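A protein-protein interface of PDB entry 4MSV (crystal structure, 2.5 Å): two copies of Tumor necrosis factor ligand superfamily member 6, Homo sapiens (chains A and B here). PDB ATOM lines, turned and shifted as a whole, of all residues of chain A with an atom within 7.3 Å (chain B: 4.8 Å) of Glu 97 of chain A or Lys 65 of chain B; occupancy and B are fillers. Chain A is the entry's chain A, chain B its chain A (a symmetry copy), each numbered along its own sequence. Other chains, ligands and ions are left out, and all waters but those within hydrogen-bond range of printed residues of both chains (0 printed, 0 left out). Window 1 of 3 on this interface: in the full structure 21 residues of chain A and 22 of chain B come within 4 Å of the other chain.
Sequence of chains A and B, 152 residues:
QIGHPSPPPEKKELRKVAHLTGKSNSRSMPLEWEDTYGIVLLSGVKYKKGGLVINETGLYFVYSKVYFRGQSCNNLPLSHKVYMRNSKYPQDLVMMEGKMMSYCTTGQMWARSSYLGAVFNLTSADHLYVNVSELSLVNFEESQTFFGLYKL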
ATOM      1  N   SER A  79      12.939  11.413   1.888  1.00  0.00           N
ATOM      2  CA  SER A  79      12.915  11.809   3.273  1.00  0.00           C
ATOM      3  C   SER A  79      12.280  13.186   3.274  1.00  0.00           C
ATOM      4  O   SER A  79      12.462  13.929   2.377  1.00  0.00           O
ATOM      5  CB  SER A  79      14.373  11.811   3.758  1.00  0.00           C
ATOM      6  OG  SER A  79      14.552  12.656   4.812  1.00  0.00           O
ATOM      7  N   HIS A  80      11.500  13.520   4.258  1.00  0.00           N
ATOM      8  CA  HIS A  80      10.909  14.844   4.338  1.00  0.00           C
ATOM      9  C   HIS A  80      10.885  15.240   5.817  1.00  0.00           C
ATOM     10  O   HIS A  80      10.406  14.484   6.636  1.00  0.00           O
ATOM     11  CB  HIS A  80       9.502  14.729   3.679  1.00  0.00           C
ATOM     12  CG  HIS A  80       8.612  15.906   3.868  1.00  0.00           C
ATOM     13  ND1 HIS A  80       7.260  15.762   4.009  1.00  0.00           N
ATOM     14  CD2 HIS A  80       8.865  17.229   4.000  1.00  0.00           C
ATOM     15  CE1 HIS A  80       6.697  16.960   4.142  1.00  0.00           C
ATOM     16  NE2 HIS A  80       7.650  17.873   4.163  1.00  0.00           N
ATOM     17  N   LYS A  81      11.403  16.395   6.159  1.00  0.00           N
ATOM     18  CA  LYS A  81      11.551  16.733   7.545  1.00  0.00           C
ATOM     19  C   LYS A  81      11.139  18.140   7.726  1.00  0.00           C
ATOM     20  O   LYS A  81      11.516  18.965   6.882  1.00  0.00           O
ATOM     21  CB  LYS A  81      13.014  16.752   7.983  1.00  0.00           C
ATOM     22  CG  LYS A  81      13.862  15.510   7.871  1.00  0.00           C
ATOM     23  CD  LYS A  81      15.306  15.824   8.289  1.00  0.00           C
ATOM     24  CE  LYS A  81      16.074  14.653   8.931  1.00  0.00           C
ATOM     25  NZ  LYS A  81      16.645  13.620   8.009  1.00  0.00           N
ATOM     26  N   VAL A  82      10.481  18.442   8.850  1.00  0.00           N
ATOM     27  CA  VAL A  82      10.316  19.809   9.327  1.00  0.00           C
ATOM     28  C   VAL A  82      11.169  19.964  10.545  1.00  0.00           C
ATOM     29  O   VAL A  82      11.084  19.155  11.463  1.00  0.00           O
ATOM     30  CB  VAL A  82       8.894  20.097   9.779  1.00  0.00           C
ATOM     31  CG1 VAL A  82       8.758  21.498  10.278  1.00  0.00           C
ATOM     32  CG2 VAL A  82       7.960  19.903   8.651  1.00  0.00           C
ATOM     33  N   VAL A  94      14.624  18.145  14.954  1.00  0.00           N
ATOM     34  CA  VAL A  94      13.588  17.647  14.018  1.00  0.00           C
ATOM     35  C   VAL A  94      12.255  17.546  14.705  1.00  0.00           C
ATOM     36  O   VAL A  94      12.135  16.936  15.700  1.00  0.00           O
ATOM     37  CB  VAL A  94      13.936  16.257  13.503  1.00  0.00           C
ATOM     38  CG1 VAL A  94      12.864  15.725  12.549  1.00  0.00           C
ATOM     39  CG2 VAL A  94      15.258  16.320  12.723  1.00  0.00           C
ATOM     40  N   MET A  95      11.233  18.159  14.152  1.00  0.00           N
ATOM     41  CA  MET A  95       9.953  18.183  14.800  1.00  0.00           C
ATOM     42  C   MET A  95       9.117  17.063  14.219  1.00  0.00           C
ATOM     43  O   MET A  95       8.383  16.420  14.956  1.00  0.00           O
ATOM     44  CB  MET A  95       9.329  19.520  14.566  1.00  0.00           C
ATOM     45  CG  MET A  95      10.091  20.673  15.252  1.00  0.00           C
ATOM     46  SD  MET A  95       9.733  22.248  14.399  1.00  0.00           S
ATOM     47  CE  MET A  95       7.955  22.512  14.640  1.00  0.00           C
ATOM     48  N   MET A  96       9.217  16.820  12.913  1.00  0.00           N
ATOM     49  CA  MET A  96       8.473  15.736  12.275  1.00  0.00           C
ATOM     50  C   MET A  96       9.190  15.338  11.017  1.00  0.00           C
ATOM     51  O   MET A  96       9.817  16.156  10.377  1.00  0.00           O
ATOM     52  CB  MET A  96       7.024  16.133  11.845  1.00  0.00           C
ATOM     53  CG  MET A  96       6.271  17.117  12.670  1.00  0.00           C
ATOM     54  SD  MET A  96       4.755  17.674  11.916  1.00  0.00           S
ATOM     55  CE  MET A  96       5.202  19.069  10.958  1.00  0.00           C
ATOM     56  N   GLU A  97       8.961  14.126  10.573  1.00  0.00           N
ATOM     57  CA  GLU A  97       9.734  13.568   9.514  1.00  0.00           C
ATOM     58  C   GLU A  97       9.023  12.345   9.014  1.00  0.00           C
ATOM     59  O   GLU A  97       8.413  11.624   9.782  1.00  0.00           O
ATOM     60  CB  GLU A  97      11.032  13.160  10.155  1.00  0.00           C
ATOM     61  CG  GLU A  97      12.073  12.399   9.387  1.00  0.00           C
ATOM     62  CD  GLU A  97      13.327  12.152  10.246  1.00  0.00           C
ATOM     63  OE1 GLU A  97      13.317  12.206  11.541  1.00  0.00           O
ATOM     64  OE2 GLU A  97      14.358  11.910   9.600  1.00  0.00           O
ATOM     65  N   GLY A  98       9.104  12.126   7.722  1.00  0.00           N
ATOM     66  CA  GLY A  98       8.683  10.914   7.121  1.00  0.00           C
ATOM     67  C   GLY A  98       9.732  10.444   6.129  1.00  0.00           C
ATOM     68  O   GLY A  98      10.380  11.239   5.536  1.00  0.00           O
ATOM     69  N   LYS A  99       9.903   9.139   5.968  1.00  0.00           N
ATOM     70  CA  LYS A  99      10.797   8.552   4.991  1.00  0.00           C
ATOM     71  C   LYS A  99      10.013   7.538   4.126  1.00  0.00           C
ATOM     72  O   LYS A  99       9.184   6.824   4.631  1.00  0.00           O
ATOM     73  CB  LYS A  99      12.015   7.958   5.723  1.00  0.00           C
ATOM     74  CG  LYS A  99      13.075   7.417   4.761  1.00  0.00           C
ATOM     75  CD  LYS A  99      14.522   7.920   4.942  1.00  0.00           C
ATOM     76  CE  LYS A  99      15.236   7.366   6.179  1.00  0.00           C
ATOM     77  NZ  LYS A  99      16.507   6.727   5.742  1.00  0.00           N
ATOM     78  N   SER A 114       4.227  13.293   0.684  1.00  0.00           N
ATOM     79  CA  SER A 114       4.456  13.042   2.106  1.00  0.00           C
ATOM     80  C   SER A 114       3.774  14.194   2.802  1.00  0.00           C
ATOM     81  O   SER A 114       3.990  15.364   2.418  1.00  0.00           O
ATOM     82  CB  SER A 114       5.955  12.993   2.406  1.00  0.00           C
ATOM     83  OG  SER A 114       6.294  13.414   3.740  1.00  0.00           O
ATOM     84  N   TYR A 115       2.968  13.865   3.822  1.00  0.00           N
ATOM     85  CA  TYR A 115       2.204  14.837   4.612  1.00  0.00           C
ATOM     86  C   TYR A 115       2.594  14.790   6.085  1.00  0.00           C
ATOM     87  O   TYR A 115       2.682  13.705   6.673  1.00  0.00           O
ATOM     88  CB  TYR A 115       0.678  14.676   4.446  1.00  0.00           C
ATOM     89  CG  TYR A 115      -0.057  15.863   5.095  1.00  0.00           C
ATOM     90  CD1 TYR A 115      -0.418  15.831   6.398  1.00  0.00           C
ATOM     91  CD2 TYR A 115      -0.366  16.982   4.367  1.00  0.00           C
ATOM     92  CE1 TYR A 115      -1.009  16.882   6.994  1.00  0.00           C
ATOM     93  CE2 TYR A 115      -0.990  18.064   4.943  1.00  0.00           C
ATOM     94  CZ  TYR A 115      -1.271  18.022   6.259  1.00  0.00           C
ATOM     95  OH  TYR A 115      -1.869  19.105   6.849  1.00  0.00           O
ATOM     96  N   LEU A 116       2.822  15.982   6.686  1.00  0.00           N
ATOM     97  CA  LEU A 116       3.177  16.083   8.075  1.00  0.00           C
ATOM     98  C   LEU A 116       2.411  17.214   8.717  1.00  0.00           C
ATOM     99  O   LEU A 116       2.307  18.284   8.171  1.00  0.00           O
ATOM    100  CB  LEU A 116       4.634  16.379   8.241  1.00  0.00           C
ATOM    101  CG  LEU A 116       5.619  15.447   7.600  1.00  0.00           C
ATOM    102  CD1 LEU A 116       7.002  16.072   7.576  1.00  0.00           C
ATOM    103  CD2 LEU A 116       5.669  14.198   8.401  1.00  0.00           C
ATOM    104  N   GLY A 117       1.844  16.977   9.888  1.00  0.00           N
ATOM    105  CA  GLY A 117       1.192  18.035  10.602  1.00  0.00           C
ATOM    106  C   GLY A 117       1.083  17.679  12.053  1.00  0.00           C
ATOM    107  O   GLY A 117       0.677  16.597  12.394  1.00  0.00           O
ATOM    108  N   TYR B  63      -5.143  13.920  15.661  1.00  0.00           N
ATOM    109  CA  TYR B  63      -4.226  13.507  14.583  1.00  0.00           C
ATOM    110  C   TYR B  63      -3.257  12.453  15.053  1.00  0.00           C
ATOM    111  O   TYR B  63      -3.005  12.345  16.249  1.00  0.00           O
ATOM    112  CB  TYR B  63      -3.452  14.671  14.032  1.00  0.00           C
ATOM    113  CG  TYR B  63      -2.572  15.332  15.010  1.00  0.00           C
ATOM    114  CD1 TYR B  63      -1.275  14.838  15.263  1.00  0.00           C
ATOM    115  CD2 TYR B  63      -2.951  16.474  15.644  1.00  0.00           C
ATOM    116  CE1 TYR B  63      -0.392  15.470  16.145  1.00  0.00           C
ATOM    117  CE2 TYR B  63      -2.110  17.091  16.587  1.00  0.00           C
ATOM    118  CZ  TYR B  63      -0.848  16.578  16.840  1.00  0.00           C
ATOM    119  OH  TYR B  63       0.013  17.185  17.707  1.00  0.00           O
ATOM    120  N   SER B  64      -2.791  11.632  14.122  1.00  0.00           N
ATOM    121  CA  SER B  64      -1.804  10.680  14.446  1.00  0.00           C
ATOM    122  C   SER B  64      -1.008  10.292  13.222  1.00  0.00           C
ATOM    123  O   SER B  64      -1.536  10.129  12.148  1.00  0.00           O
ATOM    124  CB  SER B  64      -2.432   9.416  15.033  1.00  0.00           C
ATOM    125  OG  SER B  64      -1.430   8.428  15.280  1.00  0.00           O
ATOM    126  N   LYS B  65       0.273  10.038  13.437  1.00  0.00           N
ATOM    127  CA  LYS B  65       1.106   9.516  12.401  1.00  0.00           C
ATOM    128  C   LYS B  65       1.808   8.307  12.891  1.00  0.00           C
ATOM    129  O   LYS B  65       2.392   8.347  13.981  1.00  0.00           O
ATOM    130  CB  LYS B  65       2.158  10.588  12.033  1.00  0.00           C
ATOM    131  CG  LYS B  65       3.183  10.123  11.023  1.00  0.00           C
ATOM    132  CD  LYS B  65       4.141  11.267  10.663  1.00  0.00           C
ATOM    133  CE  LYS B  65       4.996  10.958   9.431  1.00  0.00           C
ATOM    134  NZ  LYS B  65       5.918   9.792   9.659  1.00  0.00           N
ATOM    135  N   VAL B  66       1.807   7.254  12.097  1.00  0.00           N
ATOM    136  CA  VAL B  66       2.670   6.180  12.410  1.00  0.00           C
ATOM    137  C   VAL B  66       3.553   5.731  11.295  1.00  0.00           C
ATOM    138  O   VAL B  66       3.162   5.664  10.155  1.00  0.00           O
ATOM    139  CB  VAL B  66       2.068   4.985  13.199  1.00  0.00           C
ATOM    140  CG1 VAL B  66       0.758   5.262  13.851  1.00  0.00           C
ATOM    141  CG2 VAL B  66       2.122   3.723  12.487  1.00  0.00           C
ATOM    142  N   TYR B  67       4.801   5.519  11.684  1.00  0.00           N
ATOM    143  CA  TYR B  67       5.863   5.197  10.773  1.00  0.00           C
ATOM    144  C   TYR B  67       6.174   3.719  10.816  1.00  0.00           C
ATOM    145  O   TYR B  67       6.519   3.200  11.840  1.00  0.00           O
ATOM    146  CB  TYR B  67       7.075   5.990  11.208  1.00  0.00           C
ATOM    147  CG  TYR B  67       8.299   5.783  10.385  1.00  0.00           C
ATOM    148  CD1 TYR B  67       8.248   5.745   9.021  1.00  0.00           C
ATOM    149  CD2 TYR B  67       9.524   5.712  10.989  1.00  0.00           C
ATOM    150  CE1 TYR B  67       9.390   5.603   8.275  1.00  0.00           C
ATOM    151  CE2 TYR B  67      10.671   5.585  10.264  1.00  0.00           C
ATOM    152  CZ  TYR B  67      10.606   5.525   8.919  1.00  0.00           C
ATOM    153  OH  TYR B  67      11.772   5.363   8.231  1.00  0.00           O
ATOM    154  N   HIS B  80      -3.970   1.350  10.502  1.00  0.00           N
ATOM    155  CA  HIS B  80      -3.724   2.330  11.544  1.00  0.00           C
ATOM    156  C   HIS B  80      -5.071   2.967  11.894  1.00  0.00           C
ATOM    157  O   HIS B  80      -5.772   3.418  11.013  1.00  0.00           O
ATOM    158  CB  HIS B  80      -2.672   3.322  10.966  1.00  0.00           C
ATOM    159  CG  HIS B  80      -2.449   4.554  11.768  1.00  0.00           C
ATOM    160  ND1 HIS B  80      -2.173   5.754  11.172  1.00  0.00           N
ATOM    161  CD2 HIS B  80      -2.516   4.802  13.097  1.00  0.00           C
ATOM    162  CE1 HIS B  80      -1.998   6.684  12.107  1.00  0.00           C
ATOM    163  NE2 HIS B  80      -2.222   6.142  13.289  1.00  0.00           N
ATOM    164  N   SER B 113       4.766   5.908   6.011  1.00  0.00           N
ATOM    165  CA  SER B 113       3.974   6.376   7.135  1.00  0.00           C
ATOM    166  C   SER B 113       2.472   6.441   6.798  1.00  0.00           C
ATOM    167  O   SER B 113       2.061   6.460   5.607  1.00  0.00           O
ATOM    168  CB  SER B 113       4.422   7.767   7.563  1.00  0.00           C
ATOM    169  OG  SER B 113       5.747   7.729   8.035  1.00  0.00           O
ATOM    170  N   SER B 114       1.662   6.544   7.853  1.00  0.00           N
ATOM    171  CA  SER B 114       0.221   6.730   7.680  1.00  0.00           C
ATOM    172  C   SER B 114      -0.102   7.937   8.526  1.00  0.00           C
ATOM    173  O   SER B 114       0.314   7.998   9.703  1.00  0.00           O
ATOM    174  CB  SER B 114      -0.536   5.485   8.140  1.00  0.00           C
ATOM    175  OG  SER B 114      -1.859   5.760   8.639  1.00  0.00           O
ATOM    176  N   TYR B 115      -0.845   8.883   7.932  1.00  0.00           N
ATOM    177  CA  TYR B 115      -1.250  10.136   8.579  1.00  0.00           C
ATOM    178  C   TYR B 115      -2.768  10.261   8.652  1.00  0.00           C
ATOM    179  O   TYR B 115      -3.464  10.026   7.656  1.00  0.00           O
ATOM    180  CB  TYR B 115      -0.631  11.381   7.911  1.00  0.00           C
ATOM    181  CG  TYR B 115      -0.891  12.632   8.770  1.00  0.00           C
ATOM    182  CD1 TYR B 115      -2.011  13.372   8.605  1.00  0.00           C
ATOM    183  CD2 TYR B 115       0.009  13.028   9.725  1.00  0.00           C
ATOM    184  CE1 TYR B 115      -2.279  14.433   9.387  1.00  0.00           C
ATOM    185  CE2 TYR B 115      -0.227  14.122  10.525  1.00  0.00           C
ATOM    186  CZ  TYR B 115      -1.385  14.792  10.377  1.00  0.00           C
ATOM    187  OH  TYR B 115      -1.642  15.867  11.186  1.00  0.00           O
ATOM    188  N   GLU B 141      10.537   6.531  16.779  1.00  0.00           N
ATOM    189  CA  GLU B 141      11.172   7.822  16.890  1.00  0.00           C
ATOM    190  C   GLU B 141      10.161   8.943  17.073  1.00  0.00           C
ATOM    191  O   GLU B 141       9.110   8.961  16.450  1.00  0.00           O
ATOM    192  CB  GLU B 141      12.057   8.023  15.661  1.00  0.00           C
ATOM    193  CG  GLU B 141      13.284   7.077  15.694  1.00  0.00           C
ATOM    194  CD  GLU B 141      14.025   7.016  14.356  1.00  0.00           C
ATOM    195  OE1 GLU B 141      14.509   5.924  13.915  1.00  0.00           O
ATOM    196  OE2 GLU B 141      14.097   8.068  13.701  1.00  0.00           O
ATOM    197  N   SER B 143       9.880  12.012  16.192  1.00  0.00           N
ATOM    198  CA  SER B 143       9.503  12.862  15.076  1.00  0.00           C
ATOM    199  C   SER B 143       8.734  12.087  13.992  1.00  0.00           C
ATOM    200  O   SER B 143       8.271  12.643  13.038  1.00  0.00           O
ATOM    201  CB  SER B 143      10.797  13.469  14.462  1.00  0.00           C
ATOM    202  OG  SER B 143      11.643  12.431  13.919  1.00  0.00           O
ATOM    203  N   GLN B 144       8.722  10.778  14.095  1.00  0.00           N
ATOM    204  CA  GLN B 144       8.160   9.870  13.064  1.00  0.00           C
ATOM    205  C   GLN B 144       6.799   9.310  13.442  1.00  0.00           C
ATOM    206  O   GLN B 144       5.969   9.181  12.558  1.00  0.00           O
ATOM    207  CB  GLN B 144       9.064   8.736  12.851  1.00  0.00           C
ATOM    208  CG  GLN B 144      10.330   9.160  12.112  1.00  0.00           C
ATOM    209  CD  GLN B 144      10.217   8.894  10.610  1.00  0.00           C
ATOM    210  OE1 GLN B 144       9.101   8.691  10.024  1.00  0.00           O
ATOM    211  NE2 GLN B 144      11.371   8.862   9.971  1.00  0.00           N
ATOM    212  N   THR B 145       6.579   9.030  14.720  1.00  0.00           N
ATOM    213  CA  THR B 145       5.382   8.391  15.180  1.00  0.00           C
ATOM    214  C   THR B 145       4.773   9.141  16.341  1.00  0.00           C
ATOM    215  O   THR B 145       5.442   9.390  17.293  1.00  0.00           O
ATOM    216  CB  THR B 145       5.679   6.966  15.556  1.00  0.00           C
ATOM    217  OG1 THR B 145       5.990   6.226  14.366  1.00  0.00           O
ATOM    218  CG2 THR B 145       4.455   6.294  16.213  1.00  0.00           C
ATOM    219  N   PHE B 146       3.533   9.610  16.225  1.00  0.00           N
ATOM    220  CA  PHE B 146       2.972  10.475  17.248  1.00  0.00           C
ATOM    221  C   PHE B 146       1.475  10.512  17.202  1.00  0.00           C
ATOM    222  O   PHE B 146       0.847   9.922  16.278  1.00  0.00           O
ATOM    223  CB  PHE B 146       3.551  11.878  17.132  1.00  0.00           C
ATOM    224  CG  PHE B 146       3.450  12.512  15.767  1.00  0.00           C
ATOM    225  CD1 PHE B 146       2.250  13.005  15.296  1.00  0.00           C
ATOM    226  CD2 PHE B 146       4.590  12.742  15.008  1.00  0.00           C
ATOM    227  CE1 PHE B 146       2.184  13.651  14.089  1.00  0.00           C
ATOM    228  CE2 PHE B 146       4.520  13.351  13.761  1.00  0.00           C
ATOM    229  CZ  PHE B 146       3.303  13.802  13.302  1.00  0.00           C
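The backbone carbonyl oxygen (O) of Glu 97 of chain A lies close to the side-chain amide oxygen (OE1) of Gln 144 of chain B (3.0 Å). The side-chain carboxylate (OE1) of Glu 97 of chain A sits at hydrogen-bond distance from the side-chain hydroxyl (OG) of Ser 143 of chain B (2.9 Å). O of Glu 97 of chain A lies within hydrogen-bond range of NZ of Lys 65 of chain B. The backbone carbonyl oxygen (O) of Gly 117 of chain A sits at hydrogen-bond distance from the side-chain hydroxyl (OH) of Tyr 115 of chain B.
The backbone carbonyl oxygen (O) of Met 96 of chain A sits at hydrogen-bond distance from the backbone NH (N) of Val 82 of chain A (2.8 Å). O of Gln 144 of chain B sits at hydrogen-bond distance from NZ of Lys 65 of chain B. NZ of Lys 81 of chain A lies within salt-bridge range of OE2 of Glu 97 of chain A (3.3 Å). N of His 80 of chain A sits at hydrogen-bond distance from O of Gly 98 of chain A (2.8 Å). The backbone NH (N) of Gly 117 of chain A is in hydrogen-bond range of the side-chain sulfur (SD) of Met 96 of chain A (3.6 Å). NZ of Lys 65 of chain B is in hydrogen-bond range of OG of Ser 113 of chain B.
Among the printed residues, merely in contact across the chains: Val 94 of chain A with Ser 143 of chain B (3.6 Å), Met 95 of chain A with Ser 143 of chain B (3.7 Å), Met 96 of chain A with Ser 143 of chain B (3.2 Å), Gly 98 of chain A with Lys 65 of chain B (3.9 Å), Gly 98 of chain A with Gln 144 of chain B (3.7 Å), Lys 99 of chain A with Tyr 67 of chain B (3.6 Å), Tyr 115 of chain A with Tyr 115 of chain B (3.7 Å), Leu 116 of chain A with Lys 65 of chain B (3.5 Å), Gly 117 of chain A with Tyr 63 of chain B (3.9 Å) and Gly 117 of chain A with Phe 146 of chain B (3.7 Å).
Val 82 of chain A touches none of the printed residues of chain B. Of the printed residues of chain B, Val 94 of chain A touches Ser 143 (3.6 Å). Of the printed residues of chain B, Met 95 of chain A touches Ser 143 (3.7 Å). Of chain B, only Lys 65, Ser 143 and Gln 144 come within 4 Å of Glu 97 of chain A. Of the printed residues of chain B, Gly 98 of chain A touches Lys 65 (3.9 Å) and Gln 144 (3.7 Å). Lys 65 of chain B touches three residues of chain A. The nearest residue of chain B that does not touch Glu 97 of chain A is Glu 141 of chain B (4.7 Å).
Of the 14 printed residues of chain B, 7 touch a printed residue of chain A. Hydrophobic or aromatic side chains of chain B within 4 Å of the printed part of chain A: Tyr 63, Tyr 67, Tyr 115 and Phe 146. Along chain B the printed residues that touch a printed residue of chain A span positions 63 to 146. Of the 14 printed residues of chain A, 9 touch a printed residue of chain B. Printed residues of chain A that touch a printed residue of chain B: Val 94, Met 95, Met 96, Glu 97, Gly 98, Lys 99, Tyr 115, Leu 116 and Gly 117. Hydrophobic or aromatic side chains of chain A within 4 Å of the printed part of chain B: Val 94, Met 96, Tyr 115 and Leu 116. Among the printed residues, no Asp or Glu carboxylate lies within 4 Å of a Lys or Arg side-chain nitrogen of the other chain.
Tyr 115 of chain A touches its own counterpart, Tyr 115 of chain B.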
